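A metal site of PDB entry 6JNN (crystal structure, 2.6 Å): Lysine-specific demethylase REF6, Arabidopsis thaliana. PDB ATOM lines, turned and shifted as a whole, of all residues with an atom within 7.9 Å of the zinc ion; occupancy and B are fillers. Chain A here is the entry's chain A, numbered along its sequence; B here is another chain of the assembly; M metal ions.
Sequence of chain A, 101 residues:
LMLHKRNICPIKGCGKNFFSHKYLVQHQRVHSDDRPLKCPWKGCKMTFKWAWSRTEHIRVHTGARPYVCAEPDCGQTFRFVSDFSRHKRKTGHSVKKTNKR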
ATOM      1  N   LYS A  38      17.160  22.258 -27.331  1.00  0.00           N
ATOM      2  CA  LYS A  38      16.779  23.495 -28.052  1.00  0.00           C
ATOM      3  C   LYS A  38      15.739  24.237 -27.262  1.00  0.00           C
ATOM      4  O   LYS A  38      14.864  23.603 -26.618  1.00  0.00           O
ATOM      5  CB  LYS A  38      16.306  23.207 -29.508  1.00  0.00           C
ATOM      6  CG  LYS A  38      17.193  22.161 -30.203  1.00  0.00           C
ATOM      7  CD  LYS A  38      18.520  22.798 -30.636  1.00  0.00           C
ATOM      8  CE  LYS A  38      19.610  21.806 -31.042  1.00  0.00           C
ATOM      9  NZ  LYS A  38      20.750  22.484 -31.696  1.00  0.00           N
ATOM     10  N   CYS A  39      15.797  25.557 -27.290  1.00  0.00           N
ATOM     11  CA  CYS A  39      14.676  26.363 -26.800  1.00  0.00           C
ATOM     12  C   CYS A  39      13.460  26.048 -27.638  1.00  0.00           C
ATOM     13  O   CYS A  39      13.577  25.869 -28.856  1.00  0.00           O
ATOM     14  CB  CYS A  39      14.964  27.850 -26.932  1.00  0.00           C
ATOM     15  SG  CYS A  39      13.681  28.878 -26.154  1.00  0.00           S
ATOM     16  N   PRO A  40      12.295  25.891 -26.981  1.00  0.00           N
ATOM     17  CA  PRO A  40      11.077  25.553 -27.720  1.00  0.00           C
ATOM     18  C   PRO A  40      10.348  26.800 -28.230  1.00  0.00           C
ATOM     19  O   PRO A  40       9.305  26.670 -28.905  1.00  0.00           O
ATOM     20  CB  PRO A  40      10.245  24.824 -26.675  1.00  0.00           C
ATOM     21  CG  PRO A  40      10.695  25.371 -25.358  1.00  0.00           C
ATOM     22  CD  PRO A  40      12.129  25.758 -25.521  1.00  0.00           C
ATOM     23  N   TRP A  41      10.830  27.990 -27.880  1.00  0.00           N
ATOM     24  CA  TRP A  41      10.105  29.211 -28.238  1.00  0.00           C
ATOM     25  C   TRP A  41      10.378  29.625 -29.651  1.00  0.00           C
ATOM     26  O   TRP A  41      11.546  29.626 -30.057  1.00  0.00           O
ATOM     27  CB  TRP A  41      10.500  30.347 -27.342  1.00  0.00           C
ATOM     28  CG  TRP A  41       9.403  31.301 -27.085  1.00  0.00           C
ATOM     29  CD1 TRP A  41       9.195  32.480 -27.698  1.00  0.00           C
ATOM     30  CD2 TRP A  41       8.402  31.167 -26.068  1.00  0.00           C
ATOM     31  NE1 TRP A  41       8.089  33.100 -27.135  1.00  0.00           N
ATOM     32  CE2 TRP A  41       7.594  32.323 -26.139  1.00  0.00           C
ATOM     33  CE3 TRP A  41       8.122  30.195 -25.105  1.00  0.00           C
ATOM     34  CZ2 TRP A  41       6.498  32.525 -25.292  1.00  0.00           C
ATOM     35  CZ3 TRP A  41       7.024  30.386 -24.246  1.00  0.00           C
ATOM     36  CH2 TRP A  41       6.235  31.537 -24.342  1.00  0.00           C
ATOM     37  N   LYS A  42       9.323  29.947 -30.410  1.00  0.00           N
ATOM     38  CA  LYS A  42       9.487  30.217 -31.835  1.00  0.00           C
ATOM     39  C   LYS A  42      10.497  31.347 -32.076  1.00  0.00           C
ATOM     40  O   LYS A  42      10.441  32.397 -31.438  1.00  0.00           O
ATOM     41  CB  LYS A  42       8.156  30.452 -32.547  1.00  0.00           C
ATOM     42  CG  LYS A  42       7.512  29.148 -33.031  1.00  0.00           C
ATOM     43  CD  LYS A  42       6.221  29.372 -33.837  1.00  0.00           C
ATOM     44  CE  LYS A  42       5.513  28.076 -34.168  1.00  0.00           C
ATOM     45  NZ  LYS A  42       4.058  28.314 -34.468  1.00  0.00           N
ATOM     46  N   GLY A  43      11.424  31.079 -32.994  1.00  0.00           N
ATOM     47  CA  GLY A  43      12.419  32.017 -33.386  1.00  0.00           C
ATOM     48  C   GLY A  43      13.488  32.361 -32.385  1.00  0.00           C
ATOM     49  O   GLY A  43      14.266  33.296 -32.611  1.00  0.00           O
ATOM     50  N   CYS A  44      13.531  31.614 -31.269  1.00  0.00           N
ATOM     51  CA  CYS A  44      14.623  31.748 -30.305  1.00  0.00           C
ATOM     52  C   CYS A  44      15.656  30.702 -30.649  1.00  0.00           C
ATOM     53  O   CYS A  44      15.329  29.537 -30.871  1.00  0.00           O
ATOM     54  CB  CYS A  44      14.132  31.611 -28.877  1.00  0.00           C
ATOM     55  SG  CYS A  44      15.469  31.479 -27.644  1.00  0.00           S
ATOM     56  N   LYS A  45      16.913  31.103 -30.715  1.00  0.00           N
ATOM     57  CA  LYS A  45      17.994  30.239 -31.160  1.00  0.00           C
ATOM     58  C   LYS A  45      18.856  29.793 -29.997  1.00  0.00           C
ATOM     59  O   LYS A  45      19.888  29.100 -30.206  1.00  0.00           O
ATOM     60  CB  LYS A  45      18.874  31.020 -32.175  1.00  0.00           C
ATOM     61  CG  LYS A  45      18.160  31.478 -33.446  1.00  0.00           C
ATOM     62  CD  LYS A  45      17.348  32.779 -33.235  1.00  0.00           C
ATOM     63  CE  LYS A  45      16.837  33.337 -34.550  1.00  0.00           C
ATOM     64  NZ  LYS A  45      15.882  32.427 -35.236  1.00  0.00           N
ATOM     65  N   MET A  46      18.471  30.133 -28.760  1.00  0.00           N
ATOM     66  CA  MET A  46      19.162  29.612 -27.574  1.00  0.00           C
ATOM     67  C   MET A  46      19.167  28.088 -27.533  1.00  0.00           C
ATOM     68  O   MET A  46      18.213  27.456 -27.933  1.00  0.00           O
ATOM     69  CB  MET A  46      18.522  30.142 -26.321  1.00  0.00           C
ATOM     70  CG  MET A  46      19.354  29.981 -25.066  1.00  0.00           C
ATOM     71  SD  MET A  46      20.666  31.143 -24.995  1.00  0.00           S
ATOM     72  CE  MET A  46      19.789  32.695 -25.128  1.00  0.00           C
ATOM     73  N   THR A  47      20.283  27.542 -27.060  1.00  0.00           N
ATOM     74  CA  THR A  47      20.466  26.088 -26.957  1.00  0.00           C
ATOM     75  C   THR A  47      21.036  25.776 -25.588  1.00  0.00           C
ATOM     76  O   THR A  47      21.552  26.676 -24.902  1.00  0.00           O
ATOM     77  CB  THR A  47      21.498  25.603 -27.966  1.00  0.00           C
ATOM     78  OG1 THR A  47      22.669  26.436 -27.856  1.00  0.00           O
ATOM     79  CG2 THR A  47      20.922  25.610 -29.379  1.00  0.00           C
ATOM     80  N   PHE A  48      20.943  24.512 -25.183  1.00  0.00           N
ATOM     81  CA  PHE A  48      21.493  24.094 -23.900  1.00  0.00           C
ATOM     82  C   PHE A  48      22.145  22.725 -23.993  1.00  0.00           C
ATOM     83  O   PHE A  48      21.949  21.986 -24.962  1.00  0.00           O
ATOM     84  CB  PHE A  48      20.436  24.134 -22.805  1.00  0.00           C
ATOM     85  CG  PHE A  48      19.576  25.322 -22.882  1.00  0.00           C
ATOM     86  CD1 PHE A  48      18.508  25.370 -23.774  1.00  0.00           C
ATOM     87  CD2 PHE A  48      19.895  26.442 -22.154  1.00  0.00           C
ATOM     88  CE1 PHE A  48      17.729  26.499 -23.875  1.00  0.00           C
ATOM     89  CE2 PHE A  48      19.106  27.580 -22.206  1.00  0.00           C
ATOM     90  CZ  PHE A  48      18.007  27.616 -23.082  1.00  0.00           C
ATOM     91  N   ARG A  54      17.267  24.815 -19.561  1.00  0.00           N
ATOM     92  CA  ARG A  54      16.174  25.034 -20.462  1.00  0.00           C
ATOM     93  C   ARG A  54      14.925  25.438 -19.697  1.00  0.00           C
ATOM     94  O   ARG A  54      14.499  26.573 -19.761  1.00  0.00           O
ATOM     95  CB  ARG A  54      15.946  23.762 -21.276  1.00  0.00           C
ATOM     96  CG  ARG A  54      15.078  23.849 -22.533  1.00  0.00           C
ATOM     97  CD  ARG A  54      14.886  22.409 -22.953  1.00  0.00           C
ATOM     98  NE  ARG A  54      14.150  22.215 -24.189  1.00  0.00           N
ATOM     99  CZ  ARG A  54      12.845  22.000 -24.296  1.00  0.00           C
ATOM    100  NH1 ARG A  54      12.060  21.998 -23.171  1.00  0.00           N
ATOM    101  NH2 ARG A  54      12.314  21.839 -25.520  1.00  0.00           N
ATOM    102  N   HIS A  57      15.232  28.855 -18.493  1.00  0.00           N
ATOM    103  CA  HIS A  57      15.272  29.811 -19.593  1.00  0.00           C
ATOM    104  C   HIS A  57      13.856  30.115 -20.097  1.00  0.00           C
ATOM    105  O   HIS A  57      13.492  31.243 -20.345  1.00  0.00           O
ATOM    106  CB  HIS A  57      16.132  29.275 -20.709  1.00  0.00           C
ATOM    107  CG  HIS A  57      15.888  29.943 -21.994  1.00  0.00           C
ATOM    108  ND1 HIS A  57      16.531  31.102 -22.405  1.00  0.00           N
ATOM    109  CD2 HIS A  57      15.080  29.578 -23.001  1.00  0.00           C
ATOM    110  CE1 HIS A  57      16.093  31.435 -23.597  1.00  0.00           C
ATOM    111  NE2 HIS A  57      15.217  30.516 -23.996  1.00  0.00           N
ATOM    112  N   ILE A  58      13.035  29.090 -20.153  1.00  0.00           N
ATOM    113  CA  ILE A  58      11.698  29.201 -20.695  1.00  0.00           C
ATOM    114  C   ILE A  58      10.900  30.277 -19.947  1.00  0.00           C
ATOM    115  O   ILE A  58      10.187  31.102 -20.576  1.00  0.00           O
ATOM    116  CB  ILE A  58      11.008  27.831 -20.696  1.00  0.00           C
ATOM    117  CG1 ILE A  58      11.688  26.921 -21.740  1.00  0.00           C
ATOM    118  CG2 ILE A  58       9.530  27.940 -21.017  1.00  0.00           C
ATOM    119  CD1 ILE A  58      11.346  25.443 -21.589  1.00  0.00           C
ATOM    120  N   VAL A  60      11.851  33.001 -18.955  1.00  0.00           N
ATOM    121  CA  VAL A  60      12.145  34.365 -19.393  1.00  0.00           C
ATOM    122  C   VAL A  60      11.165  34.731 -20.510  1.00  0.00           C
ATOM    123  O   VAL A  60      10.737  35.921 -20.586  1.00  0.00           O
ATOM    124  CB  VAL A  60      13.607  34.640 -19.788  1.00  0.00           C
ATOM    125  CG1 VAL A  60      14.588  34.054 -18.792  1.00  0.00           C
ATOM    126  CG2 VAL A  60      13.937  34.235 -21.220  1.00  0.00           C
ATOM    127  N   HIS A  61      10.765  33.735 -21.320  1.00  0.00           N
ATOM    128  CA  HIS A  61       9.739  33.998 -22.332  1.00  0.00           C
ATOM    129  C   HIS A  61       8.368  34.133 -21.692  1.00  0.00           C
ATOM    130  O   HIS A  61       7.616  35.070 -21.987  1.00  0.00           O
ATOM    131  CB  HIS A  61       9.677  32.908 -23.380  1.00  0.00           C
ATOM    132  CG  HIS A  61      10.960  32.675 -24.090  1.00  0.00           C
ATOM    133  ND1 HIS A  61      11.398  33.449 -25.128  1.00  0.00           N
ATOM    134  CD2 HIS A  61      11.855  31.672 -23.961  1.00  0.00           C
ATOM    135  CE1 HIS A  61      12.539  32.975 -25.589  1.00  0.00           C
ATOM    136  NE2 HIS A  61      12.846  31.898 -24.884  1.00  0.00           N
ATOM    137  P    DT B   4      18.864  32.383 -19.407  1.00  0.00           P
ATOM    138  OP1  DT B   4      18.688  32.570 -20.788  1.00  0.00           O
ATOM    139  OP2  DT B   4      17.852  31.850 -18.602  1.00  0.00           O
ATOM    140  O5'  DT B   4      20.115  31.480 -19.177  1.00  0.00           O
ATOM    141  C5'  DT B   4      21.350  31.860 -19.751  1.00  0.00           C
ATOM    142  C4'  DT B   4      22.494  31.021 -19.233  1.00  0.00           C
ATOM    143  O4'  DT B   4      22.677  31.285 -17.838  1.00  0.00           O
ATOM    144  C3'  DT B   4      22.369  29.515 -19.357  1.00  0.00           C
ATOM    145  O3'  DT B   4      23.626  29.017 -19.811  1.00  0.00           O
ATOM    146  C2'  DT B   4      22.112  29.072 -17.945  1.00  0.00           C
ATOM    147  C1'  DT B   4      22.890  30.077 -17.157  1.00  0.00           C
ATOM    148  N1   DT B   4      22.405  30.255 -15.812  1.00  0.00           N
ATOM    149  C2   DT B   4      23.274  30.094 -14.769  1.00  0.00           C
ATOM    150  O2   DT B   4      24.438  29.797 -14.908  1.00  0.00           O
ATOM    151  N3   DT B   4      22.727  30.312 -13.538  1.00  0.00           N
ATOM    152  C4   DT B   4      21.424  30.671 -13.252  1.00  0.00           C
ATOM    153  O4   DT B   4      21.082  30.837 -12.095  1.00  0.00           O
ATOM    154  C5   DT B   4      20.567  30.818 -14.394  1.00  0.00           C
ATOM    155  C7   DT B   4      19.140  31.179 -14.184  1.00  0.00           C
ATOM    156  C6   DT B   4      21.096  30.604 -15.608  1.00  0.00           C
HETATM  157 ZN    ZN M   1      14.516  30.826 -25.837  1.00  0.00          ZN
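A ring nitrogen (ND1) of His 57 sits at hydrogen-bond distance from OP1 of DT 4 of chain B.
The backbone carbonyl oxygen (O) of Met 46 sits at hydrogen-bond distance from the backbone NH (N) of Cys 39 (3.1 Å).
The side-chain sulfur (SG) of Cys 44 sits close to the backbone NH (N) of Met 46 (3.5 Å).
The backbone NH of Trp 41 lies close to the side-chain sulfur of Cys 39 (3.4 Å).
The zinc ion is bound by NE2 of His 57 (2.0 Å), SG of Cys 39 (2.1 Å), SG of Cys 44 (2.1 Å) and NE2 of His 61 (2.2 Å).
The zinc ion has four donor atoms within binding distance.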
